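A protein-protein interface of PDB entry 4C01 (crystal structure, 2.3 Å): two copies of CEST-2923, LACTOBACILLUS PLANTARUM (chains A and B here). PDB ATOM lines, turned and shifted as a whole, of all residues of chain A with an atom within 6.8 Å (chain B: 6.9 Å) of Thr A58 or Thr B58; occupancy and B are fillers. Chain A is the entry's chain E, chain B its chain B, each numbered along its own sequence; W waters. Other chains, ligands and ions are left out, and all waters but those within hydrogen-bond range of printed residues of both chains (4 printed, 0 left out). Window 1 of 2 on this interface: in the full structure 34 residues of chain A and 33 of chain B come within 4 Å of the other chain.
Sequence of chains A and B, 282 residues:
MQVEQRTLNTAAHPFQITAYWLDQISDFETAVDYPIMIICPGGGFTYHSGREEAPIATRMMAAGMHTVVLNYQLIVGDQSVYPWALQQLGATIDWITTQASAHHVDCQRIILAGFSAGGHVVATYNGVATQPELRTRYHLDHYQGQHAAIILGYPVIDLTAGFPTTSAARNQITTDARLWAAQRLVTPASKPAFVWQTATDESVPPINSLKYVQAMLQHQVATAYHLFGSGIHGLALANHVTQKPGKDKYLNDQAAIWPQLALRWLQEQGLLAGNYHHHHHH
The side-chain sulfur (SD) of Met A1 sits close to the side-chain sulfur (SD) of Met B1 (3.3 Å).
N of Tyr B20 sits at hydrogen-bond distance from O of Thr B67.
OG1 of Thr B58 lies within hydrogen-bond range of O of Ala B54.
The backbone NH of Tyr A20 is in hydrogen-bond range of the backbone carbonyl oxygen of Thr A67 (2.6 Å).
The side-chain hydroxyl (OG1) of Thr A58 sits at hydrogen-bond distance from the backbone carbonyl oxygen (O) of Ala A54.
CD2 of Tyr B20 touches CE of Met A1, 3.5 Å away.
Thr B58 touches Met A1.
Met B61 touches Met A1 (CE to CE, 3.6 Å).
Tyr A20 touches Met B1.
Thr A58 touches Met B1.
Thr A58 touches Thr B58.
Thr A58 touches Met B61 (CG2 to C, 3.8 Å).
CG2 of Thr A58 touches N of Ala B62, 3.6 Å away.
Thr B58 touches Met A61.
Ala A62 touches Arg B59.
Of chain B, only Met B1 (3.3 Å), Thr B58 (3.9 Å), Met B61 (3.8 Å) and Ala B62 (3.6 Å) come within 4 Å of Thr A58.
Of the printed residues of chain B, Met A61 touches Met B1 (3.7 Å) and Thr B58 (3.8 Å).
Thr A67 touches none of the printed residues of chain B.
Printed residues of chain A within 4 Å of Met B1: Met A1, Tyr A20, Thr A58 and Met A61.
Of the printed residues of chain A, Tyr B20 touches Met A1.
Leu B22 touches none of the printed residues of chain A.
Of the printed residues of chain A, Arg B59 touches Ala A62 (3.7 Å).
Of the printed residues of chain A, Ala B62 touches Thr A58 and Arg A59.
The nearest residue of chain B that does not touch Thr A58 is Leu B22 (5.8 Å).
The nearest residue of chain A that does not touch Thr B58 is Ala A63 (5.8 Å).
Of the 17 printed residues of chain A, 6 touch a printed residue of chain B.
Hydrophobic or aromatic side chains of chain A that line the printed part of chain B: Met A1, Tyr A20, Met A61 and Ala A62.
Printed residues of chain B that touch a printed residue of chain A: Met B1, Tyr B20, Thr B58, Arg B59, Met B61 and Ala B62.
Hydrophobic or aromatic side chains of chain B that line the printed part of chain A: Met B1, Tyr B20, Met B61 and Ala B62.
Among the printed residues, 14 pairs touch across the chains.
Among the printed residues, no Asp or Glu carboxylate lies within 4 Å of a Lys or Arg side-chain nitrogen of the other chain.
Met B1 touches its own counterpart, Met A1.
Met A1 touches Tyr B20, and with the chains exchanged Tyr A20 touches Met B1.
Met A1 touches Met B61, and with the chains exchanged Met A61 touches Met B1.
Thr A58 touches Ala B62, and with the chains exchanged Ala A62 touches Thr B58.
Water W3 bridges O of Pro B55 (2.6 Å) and O of Ala A62 (2.8 Å).
Water W4 lies within hydrogen-bond range of the backbone carbonyl oxygen (O) of Pro A55 (2.6 Å) and the backbone carbonyl oxygen (O) of Ala B62 (2.9 Å).
Water W2 lies within hydrogen-bond range of OH of Tyr A20 (2.8 Å) and N of Met B1 (2.9 Å).
Water W1 lies within hydrogen-bond range of NH2 of Arg B59 (3.0 Å) and NH2 of Arg A59 (3.2 Å).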
ATOM      1  N   MET A   1       2.237 -10.521  12.628  1.00  0.00           N
ATOM      2  CA  MET A   1       1.229 -10.672  11.586  1.00  0.00           C
ATOM      3  C   MET A   1       1.143 -12.133  11.141  1.00  0.00           C
ATOM      4  O   MET A   1       2.166 -12.758  10.858  1.00  0.00           O
ATOM      5  CB  MET A   1       1.573  -9.771  10.408  1.00  0.00           C
ATOM      6  CG  MET A   1       0.386  -9.342   9.591  1.00  0.00           C
ATOM      7  SD  MET A   1       0.901  -8.792   7.957  1.00  0.00           S
ATOM      8  CE  MET A   1       2.210  -7.634   8.381  1.00  0.00           C
ATOM      9  N   TYR A  20      -6.023 -12.094   7.324  1.00  0.00           N
ATOM     10  CA  TYR A  20      -4.795 -11.443   7.752  1.00  0.00           C
ATOM     11  C   TYR A  20      -4.979 -10.873   9.167  1.00  0.00           C
ATOM     12  O   TYR A  20      -5.662  -9.867   9.372  1.00  0.00           O
ATOM     13  CB  TYR A  20      -4.379 -10.347   6.765  1.00  0.00           C
ATOM     14  CG  TYR A  20      -4.213 -10.832   5.334  1.00  0.00           C
ATOM     15  CD1 TYR A  20      -3.026 -11.411   4.903  1.00  0.00           C
ATOM     16  CD2 TYR A  20      -5.251 -10.717   4.414  1.00  0.00           C
ATOM     17  CE1 TYR A  20      -2.865 -11.841   3.599  1.00  0.00           C
ATOM     18  CE2 TYR A  20      -5.100 -11.154   3.107  1.00  0.00           C
ATOM     19  CZ  TYR A  20      -3.900 -11.708   2.705  1.00  0.00           C
ATOM     20  OH  TYR A  20      -3.741 -12.148   1.404  1.00  0.00           O
ATOM     21  N   LEU A  22      -3.786  -9.141  12.576  1.00  0.00           N
ATOM     22  CA  LEU A  22      -2.839  -8.298  13.268  1.00  0.00           C
ATOM     23  C   LEU A  22      -2.317  -9.071  14.471  1.00  0.00           C
ATOM     24  O   LEU A  22      -3.051  -9.863  15.064  1.00  0.00           O
ATOM     25  CB  LEU A  22      -3.547  -7.045  13.749  1.00  0.00           C
ATOM     26  CG  LEU A  22      -3.381  -5.760  12.962  1.00  0.00           C
ATOM     27  CD1 LEU A  22      -3.342  -6.031  11.484  1.00  0.00           C
ATOM     28  CD2 LEU A  22      -4.539  -4.851  13.313  1.00  0.00           C
ATOM     29  N   ILE A  39     -13.432  -8.412   3.048  1.00  0.00           N
ATOM     30  CA  ILE A  39     -13.388  -7.876   1.690  1.00  0.00           C
ATOM     31  C   ILE A  39     -13.923  -8.863   0.641  1.00  0.00           C
ATOM     32  O   ILE A  39     -13.476 -10.023   0.575  1.00  0.00           O
ATOM     33  CB  ILE A  39     -11.960  -7.444   1.283  1.00  0.00           C
ATOM     34  CG1 ILE A  39     -11.392  -6.450   2.304  1.00  0.00           C
ATOM     35  CG2 ILE A  39     -11.970  -6.846  -0.138  1.00  0.00           C
ATOM     36  CD1 ILE A  39      -9.874  -6.194   2.186  1.00  0.00           C
ATOM     37  N   GLU A  53      -7.810  -7.530  -3.559  1.00  0.00           N
ATOM     38  CA  GLU A  53      -7.703  -8.383  -2.395  1.00  0.00           C
ATOM     39  C   GLU A  53      -6.562  -7.900  -1.474  1.00  0.00           C
ATOM     40  O   GLU A  53      -6.719  -6.909  -0.763  1.00  0.00           O
ATOM     41  CB  GLU A  53      -7.556  -9.860  -2.824  1.00  0.00           C
ATOM     42  CG  GLU A  53      -8.742 -10.388  -3.638  1.00  0.00           C
ATOM     43  CD  GLU A  53      -8.536 -11.820  -4.165  1.00  0.00           C
ATOM     44  OE1 GLU A  53      -7.412 -12.168  -4.594  1.00  0.00           O
ATOM     45  OE2 GLU A  53      -9.510 -12.600  -4.166  1.00  0.00           O
ATOM     46  N   ALA A  54      -5.426  -8.598  -1.485  1.00  0.00           N
ATOM     47  CA  ALA A  54      -4.273  -8.222  -0.668  1.00  0.00           C
ATOM     48  C   ALA A  54      -3.933  -6.717  -0.676  1.00  0.00           C
ATOM     49  O   ALA A  54      -3.789  -6.118   0.400  1.00  0.00           O
ATOM     50  CB  ALA A  54      -3.044  -9.063  -1.041  1.00  0.00           C
ATOM     51  N   PRO A  55      -3.826  -6.089  -1.872  1.00  0.00           N
ATOM     52  CA  PRO A  55      -3.433  -4.671  -1.835  1.00  0.00           C
ATOM     53  C   PRO A  55      -4.384  -3.824  -0.998  1.00  0.00           C
ATOM     54  O   PRO A  55      -3.938  -2.919  -0.277  1.00  0.00           O
ATOM     55  CB  PRO A  55      -3.505  -4.248  -3.308  1.00  0.00           C
ATOM     56  CG  PRO A  55      -3.249  -5.535  -4.101  1.00  0.00           C
ATOM     57  CD  PRO A  55      -3.924  -6.611  -3.261  1.00  0.00           C
ATOM     58  N   ILE A  56      -5.680  -4.106  -1.074  1.00  0.00           N
ATOM     59  CA  ILE A  56      -6.636  -3.344  -0.278  1.00  0.00           C
ATOM     60  C   ILE A  56      -6.592  -3.770   1.197  1.00  0.00           C
ATOM     61  O   ILE A  56      -6.633  -2.940   2.104  1.00  0.00           O
ATOM     62  CB  ILE A  56      -8.053  -3.459  -0.880  1.00  0.00           C
ATOM     63  CG1 ILE A  56      -8.048  -2.894  -2.306  1.00  0.00           C
ATOM     64  CG2 ILE A  56      -9.092  -2.757   0.003  1.00  0.00           C
ATOM     65  CD1 ILE A  56      -9.408  -2.638  -2.867  1.00  0.00           C
ATOM     66  N   ALA A  57      -6.480  -5.073   1.424  1.00  0.00           N
ATOM     67  CA  ALA A  57      -6.341  -5.596   2.774  1.00  0.00           C
ATOM     68  C   ALA A  57      -5.138  -4.960   3.490  1.00  0.00           C
ATOM     69  O   ALA A  57      -5.242  -4.505   4.644  1.00  0.00           O
ATOM     70  CB  ALA A  57      -6.216  -7.104   2.730  1.00  0.00           C
ATOM     71  N   THR A  58      -4.007  -4.907   2.798  1.00  0.00           N
ATOM     72  CA  THR A  58      -2.781  -4.399   3.398  1.00  0.00           C
ATOM     73  C   THR A  58      -2.963  -2.952   3.767  1.00  0.00           C
ATOM     74  O   THR A  58      -2.584  -2.554   4.862  1.00  0.00           O
ATOM     75  CB  THR A  58      -1.587  -4.597   2.458  1.00  0.00           C
ATOM     76  OG1 THR A  58      -1.546  -5.974   2.083  1.00  0.00           O
ATOM     77  CG2 THR A  58      -0.271  -4.254   3.136  1.00  0.00           C
ATOM     78  N   ARG A  59      -3.600  -2.169   2.898  1.00  0.00           N
ATOM     79  CA  ARG A  59      -3.790  -0.750   3.181  1.00  0.00           C
ATOM     80  C   ARG A  59      -4.716  -0.535   4.381  1.00  0.00           C
ATOM     81  O   ARG A  59      -4.555   0.430   5.133  1.00  0.00           O
ATOM     82  CB  ARG A  59      -4.302   0.002   1.950  1.00  0.00           C
ATOM     83  CG  ARG A  59      -4.529   1.509   2.199  1.00  0.00           C
ATOM     84  CD  ARG A  59      -3.221   2.187   2.571  1.00  0.00           C
ATOM     85  NE  ARG A  59      -3.371   3.576   2.993  1.00  0.00           N
ATOM     86  CZ  ARG A  59      -3.640   3.958   4.242  1.00  0.00           C
ATOM     87  NH1 ARG A  59      -3.810   3.052   5.204  1.00  0.00           N
ATOM     88  NH2 ARG A  59      -3.740   5.247   4.538  1.00  0.00           N
ATOM     89  N   MET A  60      -5.665  -1.441   4.582  1.00  0.00           N
ATOM     90  CA  MET A  60      -6.584  -1.294   5.713  1.00  0.00           C
ATOM     91  C   MET A  60      -5.900  -1.811   6.970  1.00  0.00           C
ATOM     92  O   MET A  60      -6.054  -1.231   8.043  1.00  0.00           O
ATOM     93  CB  MET A  60      -7.921  -2.024   5.480  1.00  0.00           C
ATOM     94  CG  MET A  60      -8.751  -1.475   4.331  1.00  0.00           C
ATOM     95  SD  MET A  60      -9.090   0.282   4.516  1.00  0.00           S
ATOM     96  CE  MET A  60     -10.074   0.533   3.041  1.00  0.00           C
ATOM     97  N   MET A  61      -5.140  -2.895   6.825  1.00  0.00           N
ATOM     98  CA  MET A  61      -4.326  -3.407   7.919  1.00  0.00           C
ATOM     99  C   MET A  61      -3.377  -2.359   8.471  1.00  0.00           C
ATOM    100  O   MET A  61      -3.117  -2.342   9.681  1.00  0.00           O
ATOM    101  CB  MET A  61      -3.511  -4.608   7.468  1.00  0.00           C
ATOM    102  CG  MET A  61      -4.167  -5.953   7.707  1.00  0.00           C
ATOM    103  SD  MET A  61      -2.929  -7.218   8.064  1.00  0.00           S
ATOM    104  CE  MET A  61      -1.928  -7.109   6.581  1.00  0.00           C
ATOM    105  N   ALA A  62      -2.856  -1.487   7.603  1.00  0.00           N
ATOM    106  CA  ALA A  62      -1.890  -0.465   8.041  1.00  0.00           C
ATOM    107  C   ALA A  62      -2.496   0.529   9.019  1.00  0.00           C
ATOM    108  O   ALA A  62      -1.774   1.201   9.760  1.00  0.00           O
ATOM    109  CB  ALA A  62      -1.279   0.269   6.840  1.00  0.00           C
ATOM    110  N   ALA A  63      -3.823   0.621   9.007  1.00  0.00           N
ATOM    111  CA  ALA A  63      -4.557   1.549   9.860  1.00  0.00           C
ATOM    112  C   ALA A  63      -4.988   0.838  11.144  1.00  0.00           C
ATOM    113  O   ALA A  63      -5.645   1.425  12.011  1.00  0.00           O
ATOM    114  CB  ALA A  63      -5.762   2.102   9.118  1.00  0.00           C
ATOM    115  N   GLY A  64      -4.625  -0.428  11.271  1.00  0.00           N
ATOM    116  CA  GLY A  64      -4.855  -1.114  12.525  1.00  0.00           C
ATOM    117  C   GLY A  64      -6.133  -1.920  12.573  1.00  0.00           C
ATOM    118  O   GLY A  64      -6.869  -1.878  13.567  1.00  0.00           O
ATOM    119  N   THR A  67      -8.100  -8.147   8.634  1.00  0.00           N
ATOM    120  CA  THR A  67      -8.839  -8.268   7.378  1.00  0.00           C
ATOM    121  C   THR A  67      -9.005  -9.722   6.962  1.00  0.00           C
ATOM    122  O   THR A  67      -8.156 -10.568   7.242  1.00  0.00           O
ATOM    123  CB  THR A  67      -8.150  -7.560   6.189  1.00  0.00           C
ATOM    124  OG1 THR A  67      -6.838  -8.113   6.013  1.00  0.00           O
ATOM    125  CG2 THR A  67      -8.066  -6.042   6.391  1.00  0.00           C
ATOM    126  N   MET B   1      -0.001 -12.384   0.525  1.00  0.00           N
ATOM    127  CA  MET B   1       1.094 -12.004   1.411  1.00  0.00           C
ATOM    128  C   MET B   1       1.624 -13.218   2.185  1.00  0.00           C
ATOM    129  O   MET B   1       0.835 -14.045   2.643  1.00  0.00           O
ATOM    130  CB  MET B   1       0.616 -10.919   2.360  1.00  0.00           C
ATOM    131  CG  MET B   1       1.554 -10.647   3.498  1.00  0.00           C
ATOM    132  SD  MET B   1       0.748  -9.646   4.749  1.00  0.00           S
ATOM    133  CE  MET B   1       0.013  -8.380   3.717  1.00  0.00           C
ATOM    134  N   TYR B  20       8.258 -10.038   5.453  1.00  0.00           N
ATOM    135  CA  TYR B  20       6.892  -9.972   4.933  1.00  0.00           C
ATOM    136  C   TYR B  20       6.899  -9.823   3.392  1.00  0.00           C
ATOM    137  O   TYR B  20       7.182  -8.758   2.861  1.00  0.00           O
ATOM    138  CB  TYR B  20       6.106  -8.834   5.614  1.00  0.00           C
ATOM    139  CG  TYR B  20       6.080  -8.918   7.142  1.00  0.00           C
ATOM    140  CD1 TYR B  20       7.096  -8.351   7.916  1.00  0.00           C
ATOM    141  CD2 TYR B  20       5.055  -9.571   7.801  1.00  0.00           C
ATOM    142  CE1 TYR B  20       7.070  -8.428   9.310  1.00  0.00           C
ATOM    143  CE2 TYR B  20       5.019  -9.656   9.182  1.00  0.00           C
ATOM    144  CZ  TYR B  20       6.020  -9.088   9.932  1.00  0.00           C
ATOM    145  OH  TYR B  20       5.960  -9.187  11.308  1.00  0.00           O
ATOM    146  N   LEU B  22       5.442  -9.489  -0.298  1.00  0.00           N
ATOM    147  CA  LEU B  22       4.370  -9.167  -1.221  1.00  0.00           C
ATOM    148  C   LEU B  22       4.149 -10.358  -2.157  1.00  0.00           C
ATOM    149  O   LEU B  22       5.112 -10.967  -2.624  1.00  0.00           O
ATOM    150  CB  LEU B  22       4.787  -7.951  -2.044  1.00  0.00           C
ATOM    151  CG  LEU B  22       4.110  -6.606  -1.822  1.00  0.00           C
ATOM    152  CD1 LEU B  22       3.855  -6.346  -0.372  1.00  0.00           C
ATOM    153  CD2 LEU B  22       4.963  -5.502  -2.427  1.00  0.00           C
ATOM    154  N   ILE B  39      13.877  -3.162   8.230  1.00  0.00           N
ATOM    155  CA  ILE B  39      13.643  -2.328   9.409  1.00  0.00           C
ATOM    156  C   ILE B  39      14.399  -2.805  10.650  1.00  0.00           C
ATOM    157  O   ILE B  39      14.280  -3.972  11.058  1.00  0.00           O
ATOM    158  CB  ILE B  39      12.137  -2.200   9.750  1.00  0.00           C
ATOM    159  CG1 ILE B  39      11.349  -1.697   8.531  1.00  0.00           C
ATOM    160  CG2 ILE B  39      11.939  -1.263  10.969  1.00  0.00           C
ATOM    161  CD1 ILE B  39       9.838  -1.913   8.644  1.00  0.00           C
ATOM    162  N   GLU B  53       8.078  -2.381  14.634  1.00  0.00           N
ATOM    163  CA  GLU B  53       8.256  -3.523  13.755  1.00  0.00           C
ATOM    164  C   GLU B  53       7.085  -3.661  12.781  1.00  0.00           C
ATOM    165  O   GLU B  53       7.010  -2.922  11.816  1.00  0.00           O
ATOM    166  CB  GLU B  53       8.496  -4.792  14.584  1.00  0.00           C
ATOM    167  CG  GLU B  53       9.669  -4.639  15.548  1.00  0.00           C
ATOM    168  CD  GLU B  53       9.981  -5.921  16.311  1.00  0.00           C
ATOM    169  OE1 GLU B  53       9.034  -6.599  16.781  1.00  0.00           O
ATOM    170  OE2 GLU B  53      11.180  -6.241  16.451  1.00  0.00           O
ATOM    171  N   ALA B  54       6.180  -4.606  13.034  1.00  0.00           N
ATOM    172  CA  ALA B  54       5.039  -4.839  12.149  1.00  0.00           C
ATOM    173  C   ALA B  54       4.197  -3.595  11.774  1.00  0.00           C
ATOM    174  O   ALA B  54       3.852  -3.427  10.599  1.00  0.00           O
ATOM    175  CB  ALA B  54       4.135  -5.969  12.698  1.00  0.00           C
ATOM    176  N   PRO B  55       3.858  -2.724  12.752  1.00  0.00           N
ATOM    177  CA  PRO B  55       3.023  -1.588  12.342  1.00  0.00           C
ATOM    178  C   PRO B  55       3.696  -0.721  11.275  1.00  0.00           C
ATOM    179  O   PRO B  55       3.023  -0.242  10.327  1.00  0.00           O
ATOM    180  CB  PRO B  55       2.835  -0.805  13.647  1.00  0.00           C
ATOM    181  CG  PRO B  55       2.899  -1.861  14.734  1.00  0.00           C
ATOM    182  CD  PRO B  55       3.979  -2.818  14.227  1.00  0.00           C
ATOM    183  N   ILE B  56       5.013  -0.533  11.413  1.00  0.00           N
ATOM    184  CA  ILE B  56       5.770   0.238  10.428  1.00  0.00           C
ATOM    185  C   ILE B  56       5.916  -0.548   9.120  1.00  0.00           C
ATOM    186  O   ILE B  56       5.724  -0.010   8.029  1.00  0.00           O
ATOM    187  CB  ILE B  56       7.156   0.653  10.984  1.00  0.00           C
ATOM    188  CG1 ILE B  56       6.972   1.652  12.127  1.00  0.00           C
ATOM    189  CG2 ILE B  56       8.040   1.257   9.885  1.00  0.00           C
ATOM    190  CD1 ILE B  56       8.235   2.261  12.611  1.00  0.00           C
ATOM    191  N   ALA B  57       6.241  -1.828   9.244  1.00  0.00           N
ATOM    192  CA  ALA B  57       6.320  -2.711   8.086  1.00  0.00           C
ATOM    193  C   ALA B  57       5.017  -2.724   7.275  1.00  0.00           C
ATOM    194  O   ALA B  57       5.043  -2.636   6.045  1.00  0.00           O
ATOM    195  CB  ALA B  57       6.687  -4.121   8.526  1.00  0.00           C
ATOM    196  N   THR B  58       3.881  -2.836   7.958  1.00  0.00           N
ATOM    197  CA  THR B  58       2.598  -2.914   7.268  1.00  0.00           C
ATOM    198  C   THR B  58       2.308  -1.627   6.520  1.00  0.00           C
ATOM    199  O   THR B  58       1.861  -1.666   5.368  1.00  0.00           O
ATOM    200  CB  THR B  58       1.474  -3.243   8.255  1.00  0.00           C
ATOM    201  OG1 THR B  58       1.786  -4.476   8.891  1.00  0.00           O
ATOM    202  CG2 THR B  58       0.133  -3.405   7.555  1.00  0.00           C
ATOM    203  N   ARG B  59       2.580  -0.479   7.139  1.00  0.00           N
ATOM    204  CA  ARG B  59       2.381   0.793   6.450  1.00  0.00           C
ATOM    205  C   ARG B  59       3.247   0.887   5.191  1.00  0.00           C
ATOM    206  O   ARG B  59       2.810   1.426   4.157  1.00  0.00           O
ATOM    207  CB  ARG B  59       2.657   1.968   7.380  1.00  0.00           C
ATOM    208  CG  ARG B  59       2.446   3.321   6.724  1.00  0.00           C
ATOM    209  CD  ARG B  59       1.008   3.471   6.299  1.00  0.00           C
ATOM    210  NE  ARG B  59       0.705   4.688   5.552  1.00  0.00           N
ATOM    211  CZ  ARG B  59       0.794   4.788   4.227  1.00  0.00           C
ATOM    212  NH1 ARG B  59       1.213   3.758   3.501  1.00  0.00           N
ATOM    213  NH2 ARG B  59       0.478   5.924   3.620  1.00  0.00           N
ATOM    214  N   MET B  60       4.463   0.350   5.259  1.00  0.00           N
ATOM    215  CA  MET B  60       5.333   0.391   4.092  1.00  0.00           C
ATOM    216  C   MET B  60       4.900  -0.650   3.061  1.00  0.00           C
ATOM    217  O   MET B  60       4.944  -0.385   1.863  1.00  0.00           O
ATOM    218  CB  MET B  60       6.813   0.201   4.472  1.00  0.00           C
ATOM    219  CG  MET B  60       7.386   1.306   5.338  1.00  0.00           C
ATOM    220  SD  MET B  60       7.167   2.972   4.680  1.00  0.00           S
ATOM    221  CE  MET B  60       7.539   3.894   6.173  1.00  0.00           C
ATOM    222  N   MET B  61       4.503  -1.831   3.521  1.00  0.00           N
ATOM    223  CA  MET B  61       3.984  -2.837   2.610  1.00  0.00           C
ATOM    224  C   MET B  61       2.774  -2.340   1.826  1.00  0.00           C
ATOM    225  O   MET B  61       2.589  -2.746   0.677  1.00  0.00           O
ATOM    226  CB  MET B  61       3.587  -4.092   3.362  1.00  0.00           C
ATOM    227  CG  MET B  61       4.605  -5.202   3.312  1.00  0.00           C
ATOM    228  SD  MET B  61       3.755  -6.783   3.438  1.00  0.00           S
ATOM    229  CE  MET B  61       2.969  -6.585   5.029  1.00  0.00           C
ATOM    230  N   ALA B  62       1.957  -1.478   2.445  1.00  0.00           N
ATOM    231  CA  ALA B  62       0.749  -0.945   1.804  1.00  0.00           C
ATOM    232  C   ALA B  62       1.060  -0.066   0.606  1.00  0.00           C
ATOM    233  O   ALA B  62       0.196   0.174  -0.247  1.00  0.00           O
ATOM    234  CB  ALA B  62      -0.126  -0.178   2.821  1.00  0.00           C
ATOM    235  N   ALA B  63       2.290   0.420   0.538  1.00  0.00           N
ATOM    236  CA  ALA B  63       2.709   1.247  -0.586  1.00  0.00           C
ATOM    237  C   ALA B  63       3.404   0.388  -1.643  1.00  0.00           C
ATOM    238  O   ALA B  63       3.919   0.902  -2.625  1.00  0.00           O
ATOM    239  CB  ALA B  63       3.614   2.364  -0.120  1.00  0.00           C
ATOM    240  N   GLY B  64       3.433  -0.920  -1.440  1.00  0.00           N
ATOM    241  CA  GLY B  64       3.960  -1.793  -2.470  1.00  0.00           C
ATOM    242  C   GLY B  64       5.431  -2.141  -2.373  1.00  0.00           C
ATOM    243  O   GLY B  64       6.143  -2.093  -3.385  1.00  0.00           O
ATOM    244  N   THR B  67       8.949  -6.185   3.026  1.00  0.00           N
ATOM    245  CA  THR B  67       9.650  -5.712   4.225  1.00  0.00           C
ATOM    246  C   THR B  67      10.253  -6.852   5.012  1.00  0.00           C
ATOM    247  O   THR B  67       9.749  -7.969   4.990  1.00  0.00           O
ATOM    248  CB  THR B  67       8.747  -4.984   5.229  1.00  0.00           C
ATOM    249  OG1 THR B  67       7.647  -5.837   5.572  1.00  0.00           O
ATOM    250  CG2 THR B  67       8.242  -3.659   4.682  1.00  0.00           C
HETATM  251  O   HOH W   1      -1.935   7.699   3.723  1.00  0.00           O
HETATM  252  O   HOH W   2      -2.178 -14.333   0.737  1.00  0.00           O
HETATM  253  O   HOH W   3       0.473  -0.154  10.598  1.00  0.00           O
HETATM  254  O   HOH W   4      -1.446  -2.147  -0.551  1.00  0.00           O
